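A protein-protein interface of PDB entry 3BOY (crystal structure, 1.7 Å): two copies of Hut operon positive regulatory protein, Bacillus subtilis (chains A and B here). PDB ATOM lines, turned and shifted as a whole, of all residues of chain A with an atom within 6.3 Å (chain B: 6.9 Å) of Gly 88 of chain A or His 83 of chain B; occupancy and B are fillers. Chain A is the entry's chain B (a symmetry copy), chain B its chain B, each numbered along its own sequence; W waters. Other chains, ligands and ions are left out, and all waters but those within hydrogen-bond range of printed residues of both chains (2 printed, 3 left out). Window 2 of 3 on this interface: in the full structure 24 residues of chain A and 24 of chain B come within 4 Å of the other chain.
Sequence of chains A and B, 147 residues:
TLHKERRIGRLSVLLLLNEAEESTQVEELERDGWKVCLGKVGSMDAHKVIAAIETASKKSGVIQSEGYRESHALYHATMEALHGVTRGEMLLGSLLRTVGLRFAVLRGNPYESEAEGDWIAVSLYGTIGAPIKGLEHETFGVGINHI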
ATOM      1  N   GLU A  80       7.315   0.908   4.495  1.00  0.00           N
ATOM      2  CA  GLU A  80       7.575  -0.407   5.120  1.00  0.00           C
ATOM      3  C   GLU A  80       8.061  -0.260   6.575  1.00  0.00           C
ATOM      4  O   GLU A  80       7.615  -0.967   7.480  1.00  0.00           O
ATOM      5  CB  GLU A  80       8.483  -1.267   4.218  1.00  0.00           C
ATOM      6  CG  GLU A  80       7.815  -1.621   2.855  1.00  0.00           C
ATOM      7  CD  GLU A  80       8.440  -2.809   2.071  1.00  0.00           C
ATOM      8  OE1 GLU A  80       9.306  -3.447   2.650  1.00  0.00           O
ATOM      9  N   HIS A  83       5.267   0.379   8.972  1.00  0.00           N
ATOM     10  CA  HIS A  83       4.385  -0.722   9.377  1.00  0.00           C
ATOM     11  C   HIS A  83       4.776  -1.256  10.751  1.00  0.00           C
ATOM     12  O   HIS A  83       3.912  -1.635  11.572  1.00  0.00           O
ATOM     13  CB  HIS A  83       4.409  -1.849   8.347  1.00  0.00           C
ATOM     14  CG  HIS A  83       3.344  -1.748   7.316  1.00  0.00           C
ATOM     15  ND1 HIS A  83       3.595  -1.354   6.014  1.00  0.00           N
ATOM     16  CD2 HIS A  83       2.011  -1.971   7.394  1.00  0.00           C
ATOM     17  CE1 HIS A  83       2.459  -1.339   5.338  1.00  0.00           C
ATOM     18  NE2 HIS A  83       1.484  -1.704   6.151  1.00  0.00           N
ATOM     19  N   GLY A  84       6.086  -1.301  11.004  1.00  0.00           N
ATOM     20  CA  GLY A  84       6.590  -1.855  12.240  1.00  0.00           C
ATOM     21  C   GLY A  84       6.256  -0.929  13.379  1.00  0.00           C
ATOM     22  O   GLY A  84       6.013  -1.378  14.497  1.00  0.00           O
ATOM     23  N   THR A  86       3.583   1.309  13.392  1.00  0.00           N
ATOM     24  CA  THR A  86       2.137   1.501  13.573  1.00  0.00           C
ATOM     25  C   THR A  86       1.337   0.199  13.775  1.00  0.00           C
ATOM     26  O   THR A  86       0.228   0.220  14.313  1.00  0.00           O
ATOM     27  CB  THR A  86       1.522   2.322  12.437  1.00  0.00           C
ATOM     28  OG1 THR A  86       1.751   1.701  11.175  1.00  0.00           O
ATOM     29  CG2 THR A  86       2.128   3.746  12.397  1.00  0.00           C
ATOM     30  N   ARG A  87       1.890  -0.901  13.301  1.00  0.00           N
ATOM     31  CA  ARG A  87       1.327  -2.238  13.617  1.00  0.00           C
ATOM     32  C   ARG A  87      -0.179  -2.391  13.293  1.00  0.00           C
ATOM     33  O   ARG A  87      -0.972  -2.909  14.098  1.00  0.00           O
ATOM     34  CB  ARG A  87       1.703  -2.649  15.038  1.00  0.00           C
ATOM     35  CG  ARG A  87       3.202  -2.958  15.204  1.00  0.00           C
ATOM     36  CD  ARG A  87       3.694  -2.581  16.602  1.00  0.00           C
ATOM     37  NE  ARG A  87       3.512  -1.124  16.849  1.00  0.00           N
ATOM     38  CZ  ARG A  87       2.744  -0.590  17.786  1.00  0.00           C
ATOM     39  NH1 ARG A  87       2.020  -1.352  18.635  1.00  0.00           N
ATOM     40  NH2 ARG A  87       2.641   0.734  17.848  1.00  0.00           N
ATOM     41  N   GLY A  88      -0.540  -2.004  12.077  1.00  0.00           N
ATOM     42  CA  GLY A  88      -1.831  -2.386  11.519  1.00  0.00           C
ATOM     43  C   GLY A  88      -2.646  -1.247  10.975  1.00  0.00           C
ATOM     44  O   GLY A  88      -3.370  -1.411  10.021  1.00  0.00           O
ATOM     45  N   GLU A  89      -2.503  -0.066  11.564  1.00  0.00           N
ATOM     46  CA  GLU A  89      -3.168   1.098  11.013  1.00  0.00           C
ATOM     47  C   GLU A  89      -2.144   2.226  10.957  1.00  0.00           C
ATOM     48  O   GLU A  89      -1.627   2.564  11.996  1.00  0.00           O
ATOM     49  CB  GLU A  89      -4.282   1.523  11.963  1.00  0.00           C
ATOM     50  CG  GLU A  89      -5.462   0.540  12.058  1.00  0.00           C
ATOM     51  CD  GLU A  89      -6.190   0.348  10.718  1.00  0.00           C
ATOM     52  OE1 GLU A  89      -6.697   1.340  10.072  1.00  0.00           O
ATOM     53  OE2 GLU A  89      -6.270  -0.829  10.312  1.00  0.00           O
ATOM     54  N   MET A  90      -1.876   2.784   9.772  1.00  0.00           N
ATOM     55  CA  MET A  90      -0.758   3.701   9.591  1.00  0.00           C
ATOM     56  C   MET A  90      -1.274   5.081   9.930  1.00  0.00           C
ATOM     57  O   MET A  90      -1.345   5.988   9.078  1.00  0.00           O
ATOM     58  CB  MET A  90      -0.202   3.661   8.157  1.00  0.00           C
ATOM     59  CG  MET A  90       1.290   3.923   8.153  1.00  0.00           C
ATOM     60  SD  MET A  90       2.005   3.715   6.550  1.00  0.00           S
ATOM     61  CE  MET A  90       2.297   1.947   6.585  1.00  0.00           C
ATOM     62  N   ARG A  97      -2.776   8.808  19.184  1.00  0.00           N
ATOM     63  CA  ARG A  97      -1.405   8.504  19.551  1.00  0.00           C
ATOM     64  C   ARG A  97      -0.351   9.391  18.877  1.00  0.00           C
ATOM     65  O   ARG A  97      -0.580  10.003  17.815  1.00  0.00           O
ATOM     66  CB  ARG A  97      -1.124   7.001  19.365  1.00  0.00           C
ATOM     67  CG  ARG A  97      -1.153   6.512  17.949  1.00  0.00           C
ATOM     68  CD  ARG A  97      -0.839   4.950  17.891  1.00  0.00           C
ATOM     69  NE  ARG A  97      -1.010   4.525  16.512  1.00  0.00           N
ATOM     70  CZ  ARG A  97      -0.909   3.267  16.084  1.00  0.00           C
ATOM     71  NH1 ARG A  97      -0.560   2.285  16.934  1.00  0.00           N
ATOM     72  NH2 ARG A  97      -1.148   3.026  14.791  1.00  0.00           N
ATOM     73  N   THR B  78       3.633 -11.120  19.884  1.00  0.00           N
ATOM     74  CA  THR B  78       4.163 -11.760  18.735  1.00  0.00           C
ATOM     75  C   THR B  78       3.477 -11.216  17.448  1.00  0.00           C
ATOM     76  O   THR B  78       4.162 -10.949  16.460  1.00  0.00           O
ATOM     77  CB  THR B  78       3.987 -13.289  18.806  1.00  0.00           C
ATOM     78  OG1 THR B  78       4.665 -13.751  19.987  1.00  0.00           O
ATOM     79  CG2 THR B  78       4.614 -13.932  17.607  1.00  0.00           C
ATOM     80  N   MET B  79       2.159 -11.032  17.511  1.00  0.00           N
ATOM     81  CA  MET B  79       1.397 -10.481  16.360  1.00  0.00           C
ATOM     82  C   MET B  79       1.994  -9.118  16.002  1.00  0.00           C
ATOM     83  O   MET B  79       2.226  -8.819  14.829  1.00  0.00           O
ATOM     84  CB  MET B  79      -0.086 -10.305  16.698  1.00  0.00           C
ATOM     85  CG  MET B  79      -0.827 -11.598  16.856  1.00  0.00           C
ATOM     86  SD  MET B  79      -0.865 -12.543  15.346  1.00  0.00           S
ATOM     87  CE  MET B  79       0.490 -13.620  15.602  1.00  0.00           C
ATOM     88  N   GLU B  80       2.227  -8.304  17.023  1.00  0.00           N
ATOM     89  CA  GLU B  80       2.782  -6.960  16.749  1.00  0.00           C
ATOM     90  C   GLU B  80       4.181  -7.042  16.108  1.00  0.00           C
ATOM     91  O   GLU B  80       4.493  -6.340  15.145  1.00  0.00           O
ATOM     92  CB  GLU B  80       2.697  -6.072  18.006  1.00  0.00           C
ATOM     93  CG  GLU B  80       1.228  -5.793  18.447  1.00  0.00           C
ATOM     94  CD  GLU B  80       1.016  -4.591  19.409  1.00  0.00           C
ATOM     95  OE1 GLU B  80       1.992  -3.888  19.626  1.00  0.00           O
ATOM     96  N   ALA B  81       5.044  -7.944  16.607  1.00  0.00           N
ATOM     97  CA  ALA B  81       6.350  -8.123  15.978  1.00  0.00           C
ATOM     98  C   ALA B  81       6.220  -8.589  14.535  1.00  0.00           C
ATOM     99  O   ALA B  81       6.997  -8.191  13.648  1.00  0.00           O
ATOM    100  CB  ALA B  81       7.209  -9.124  16.770  1.00  0.00           C
ATOM    101  N   LEU B  82       5.227  -9.457  14.285  1.00  0.00           N
ATOM    102  CA  LEU B  82       5.061  -9.980  12.945  1.00  0.00           C
ATOM    103  C   LEU B  82       4.641  -8.879  11.963  1.00  0.00           C
ATOM    104  O   LEU B  82       4.902  -9.018  10.778  1.00  0.00           O
ATOM    105  CB  LEU B  82       4.057 -11.130  12.934  1.00  0.00           C
ATOM    106  CG  LEU B  82       4.686 -12.437  13.385  1.00  0.00           C
ATOM    107  CD1 LEU B  82       3.538 -13.493  13.514  1.00  0.00           C
ATOM    108  CD2 LEU B  82       5.794 -12.914  12.459  1.00  0.00           C
ATOM    109  N   HIS B  83       4.050  -7.783  12.448  1.00  0.00           N
ATOM    110  CA  HIS B  83       3.677  -6.725  11.501  1.00  0.00           C
ATOM    111  C   HIS B  83       4.912  -6.135  10.829  1.00  0.00           C
ATOM    112  O   HIS B  83       4.896  -5.787   9.628  1.00  0.00           O
ATOM    113  CB  HIS B  83       2.878  -5.625  12.197  1.00  0.00           C
ATOM    114  CG  HIS B  83       1.406  -5.815  12.133  1.00  0.00           C
ATOM    115  ND1 HIS B  83       0.654  -6.227  13.218  1.00  0.00           N
ATOM    116  CD2 HIS B  83       0.538  -5.669  11.104  1.00  0.00           C
ATOM    117  CE1 HIS B  83      -0.614  -6.325  12.856  1.00  0.00           C
ATOM    118  NE2 HIS B  83      -0.711  -5.998  11.581  1.00  0.00           N
ATOM    119  N   GLY B  84       5.989  -6.007  11.607  1.00  0.00           N
ATOM    120  CA  GLY B  84       7.201  -5.393  11.111  1.00  0.00           C
ATOM    121  C   GLY B  84       7.854  -6.308  10.111  1.00  0.00           C
ATOM    122  O   GLY B  84       8.475  -5.846   9.156  1.00  0.00           O
ATOM    123  N   VAL B  85       7.709  -7.608  10.356  1.00  0.00           N
ATOM    124  CA  VAL B  85       8.263  -8.621   9.499  1.00  0.00           C
ATOM    125  C   VAL B  85       7.505  -8.732   8.166  1.00  0.00           C
ATOM    126  O   VAL B  85       8.153  -8.804   7.124  1.00  0.00           O
ATOM    127  CB  VAL B  85       8.332  -9.999  10.225  1.00  0.00           C
ATOM    128  CG1 VAL B  85       8.772 -11.125   9.259  1.00  0.00           C
ATOM    129  CG2 VAL B  85       9.283  -9.907  11.431  1.00  0.00           C
ATOM    130  N   THR B  86       6.167  -8.698   8.215  1.00  0.00           N
ATOM    131  CA  THR B  86       5.320  -8.970   7.044  1.00  0.00           C
ATOM    132  C   THR B  86       4.843  -7.712   6.291  1.00  0.00           C
ATOM    133  O   THR B  86       4.477  -7.785   5.116  1.00  0.00           O
ATOM    134  CB  THR B  86       4.122  -9.854   7.398  1.00  0.00           C
ATOM    135  OG1 THR B  86       3.324  -9.253   8.414  1.00  0.00           O
ATOM    136  CG2 THR B  86       4.590 -11.241   7.901  1.00  0.00           C
ATOM    137  N   ARG B  87       4.813  -6.594   6.991  1.00  0.00           N
ATOM    138  CA  ARG B  87       4.579  -5.285   6.331  1.00  0.00           C
ATOM    139  C   ARG B  87       3.304  -5.228   5.454  1.00  0.00           C
ATOM    140  O   ARG B  87       3.316  -4.737   4.312  1.00  0.00           O
ATOM    141  CB  ARG B  87       5.846  -4.816   5.619  1.00  0.00           C
ATOM    142  CG  ARG B  87       6.973  -4.416   6.587  1.00  0.00           C
ATOM    143  CD  ARG B  87       8.348  -4.728   5.995  1.00  0.00           C
ATOM    144  NE  ARG B  87       8.489  -6.186   5.730  1.00  0.00           N
ATOM    145  CZ  ARG B  87       8.676  -6.741   4.542  1.00  0.00           C
ATOM    146  NH1 ARG B  87       8.754  -6.002   3.414  1.00  0.00           N
ATOM    147  NH2 ARG B  87       8.729  -8.066   4.458  1.00  0.00           N
ATOM    148  N   GLY B  88       2.196  -5.667   6.036  1.00  0.00           N
ATOM    149  CA  GLY B  88       0.884  -5.375   5.471  1.00  0.00           C
ATOM    150  C   GLY B  88      -0.001  -6.573   5.279  1.00  0.00           C
ATOM    151  O   GLY B  88      -1.201  -6.476   5.404  1.00  0.00           O
ATOM    152  N   GLU B  89       0.594  -7.729   5.009  1.00  0.00           N
ATOM    153  CA  GLU B  89      -0.193  -8.943   4.933  1.00  0.00           C
ATOM    154  C   GLU B  89       0.532 -10.010   5.745  1.00  0.00           C
ATOM    155  O   GLU B  89       1.661 -10.292   5.417  1.00  0.00           O
ATOM    156  CB  GLU B  89      -0.240  -9.409   3.483  1.00  0.00           C
ATOM    157  CG  GLU B  89      -1.036  -8.494   2.535  1.00  0.00           C
ATOM    158  CD  GLU B  89      -2.519  -8.380   2.919  1.00  0.00           C
ATOM    159  OE1 GLU B  89      -3.277  -9.416   3.019  1.00  0.00           O
ATOM    160  OE2 GLU B  89      -2.938  -7.220   3.110  1.00  0.00           O
ATOM    161  N   MET B  90      -0.113 -10.582   6.767  1.00  0.00           N
ATOM    162  CA  MET B  90       0.574 -11.436   7.727  1.00  0.00           C
ATOM    163  C   MET B  90       0.548 -12.834   7.154  1.00  0.00           C
ATOM    164  O   MET B  90      -0.067 -13.766   7.710  1.00  0.00           O
ATOM    165  CB  MET B  90      -0.091 -11.400   9.114  1.00  0.00           C
ATOM    166  CG  MET B  90       0.942 -11.574  10.209  1.00  0.00           C
ATOM    167  SD  MET B  90       0.253 -11.365  11.822  1.00  0.00           S
ATOM    168  CE  MET B  90       0.376  -9.582  11.967  1.00  0.00           C
ATOM    169  N   LEU B 124      12.263  -9.829  16.480  1.00  0.00           N
ATOM    170  CA  LEU B 124      12.567 -10.746  15.377  1.00  0.00           C
ATOM    171  C   LEU B 124      13.508 -10.108  14.377  1.00  0.00           C
ATOM    172  O   LEU B 124      13.347  -8.932  14.028  1.00  0.00           O
ATOM    173  CB  LEU B 124      11.301 -11.130  14.607  1.00  0.00           C
ATOM    174  CG  LEU B 124      10.100 -11.514  15.451  1.00  0.00           C
ATOM    175  CD1 LEU B 124       8.844 -11.621  14.581  1.00  0.00           C
ATOM    176  CD2 LEU B 124      10.346 -12.870  16.134  1.00  0.00           C
ATOM    177  N   PHE B 140      12.754  -7.260  10.146  1.00  0.00           N
ATOM    178  CA  PHE B 140      12.802  -6.985  11.578  1.00  0.00           C
ATOM    179  C   PHE B 140      11.378  -6.756  12.088  1.00  0.00           C
ATOM    180  O   PHE B 140      10.506  -6.244  11.356  1.00  0.00           O
ATOM    181  CB  PHE B 140      13.459  -5.622  11.904  1.00  0.00           C
ATOM    182  CG  PHE B 140      14.927  -5.588  11.850  1.00  0.00           C
ATOM    183  CD1 PHE B 140      15.589  -5.421  10.626  1.00  0.00           C
ATOM    184  CD2 PHE B 140      15.665  -5.571  13.040  1.00  0.00           C
ATOM    185  CE1 PHE B 140      16.974  -5.313  10.569  1.00  0.00           C
ATOM    186  CE2 PHE B 140      17.063  -5.466  12.993  1.00  0.00           C
ATOM    187  CZ  PHE B 140      17.711  -5.343  11.771  1.00  0.00           C
ATOM    188  N   GLY B 141      11.163  -7.075  13.349  1.00  0.00           N
ATOM    189  CA  GLY B 141       9.894  -6.736  13.998  1.00  0.00           C
ATOM    190  C   GLY B 141      10.065  -6.713  15.493  1.00  0.00           C
ATOM    191  O   GLY B 141      10.812  -7.506  16.045  1.00  0.00           O
ATOM    192  N   VAL B 142       9.395  -5.769  16.133  1.00  0.00           N
ATOM    193  CA  VAL B 142       9.332  -5.734  17.592  1.00  0.00           C
ATOM    194  C   VAL B 142       7.909  -5.471  18.057  1.00  0.00           C
ATOM    195  O   VAL B 142       7.261  -4.523  17.582  1.00  0.00           O
ATOM    196  CB  VAL B 142      10.236  -4.595  18.123  1.00  0.00           C
ATOM    197  CG1 VAL B 142      10.143  -4.498  19.670  1.00  0.00           C
ATOM    198  CG2 VAL B 142      11.672  -4.882  17.701  1.00  0.00           C
HETATM  199  O   HOH W   1       8.460  -2.676   9.382  1.00  0.00           O
HETATM  200  O   HOH W   2       7.163  -1.772  17.096  1.00  0.00           O
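Of the printed residues of chain B, Arg 87 of chain A touches Glu 80 (2.7 Å) and His 83 (3.7 Å). Of chain B, only His 83 (3.8 Å) comes within 4 Å of Gly 88 of chain A. Arg 97 of chain A touches none of the printed residues of chain B. Printed residues of chain A within 4 Å of Glu 80 of chain B: Arg 87. Of the printed residues of chain A, His 83 of chain B touches Arg 87 (3.7 Å) and Gly 88 (3.8 Å). Printed residues of chain A within 4 Å of Gly 84 of chain B: Gly 84. Thr 86 of chain B touches none of the printed residues of chain A. Printed residues of chain A within 4 Å of Arg 87 of chain B: Glu 80 (2.7 Å) and His 83 (3.7 Å). Printed residues of chain A within 4 Å of Gly 88 of chain B: His 83. The nearest printed residue of chain B that does not touch His 83 of chain A is His 83 of chain B (4.2 Å).
Glu 80 of chain A touches Arg 87 of chain B, and with the chains exchanged Arg 87 of chain A touches Glu 80 of chain B. His 83 of chain A touches Arg 87 of chain B, and with the chains exchanged Arg 87 of chain A touches His 83 of chain B. His 83 of chain A touches Gly 88 of chain B, and with the chains exchanged Gly 88 of chain A touches His 83 of chain B. Gly 84 of chain B touches its own counterpart, Gly 84 of chain A. Positions printed for both chains: 80, 83, 84, 86, 87, 88, 89 and 90.
O of Met 79 of chain B is in hydrogen-bond range of ND1 of His 83 of chain B, at 3.4 Å. The backbone carbonyl oxygen (O) of Gly 84 of chain B lies close to the guanidinium group (NE) of Arg 87 of chain B (3.4 Å). The guanidinium group of Arg 87 of chain B is in hydrogen-bond range of the backbone carbonyl oxygen of Val 85 of chain B, 2.8 Å away. NE of Arg 87 of chain A sits close to O of Gly 84 of chain A (3.4 Å).
Among the printed residues, merely in contact across the chains: His 83 of chain A with Arg 87 of chain B, His 83 of chain A with Gly 88 of chain B, Gly 84 of chain A with Gly 84 of chain B, Arg 87 of chain A with His 83 of chain B and Gly 88 of chain A with His 83 of chain B.
Of the 17 printed residues of chain B, 5 touch a printed residue of chain A. Hydrophobic or aromatic side chains of chain B that line the printed part of chain A: His 83. Of the 9 printed residues of chain A, 5 touch a printed residue of chain B. Along chain A the printed residues that touch a printed residue of chain B span positions 80 to 88. Among the printed residues, Asp or Glu carboxylates within 4 Å of a Lys or Arg side-chain nitrogen of the other chain: Glu 80 of chain A with Arg 87 of chain B (2.7 Å) and Arg 87 of chain A with Glu 80 of chain B (2.7 Å).
OE1 of Glu 80 of chain B lies within salt-bridge range of NH1 of Arg 87 of chain A. NH1 of Arg 87 of chain B lies within salt-bridge range of OE1 of Glu 80 of chain A (2.7 Å).
Water W1 lies within hydrogen-bond range of the backbone carbonyl oxygen of Glu 80 of chain A (2.7 Å), the backbone carbonyl oxygen of Gly 84 of chain B (3.2 Å) and the backbone NH of Gly 84 of chain A (3.2 Å). Water W2 bridges the backbone carbonyl oxygen of Val 142 of chain B (2.8 Å) and the backbone carbonyl oxygen of Gly 84 of chain A (2.9 Å).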
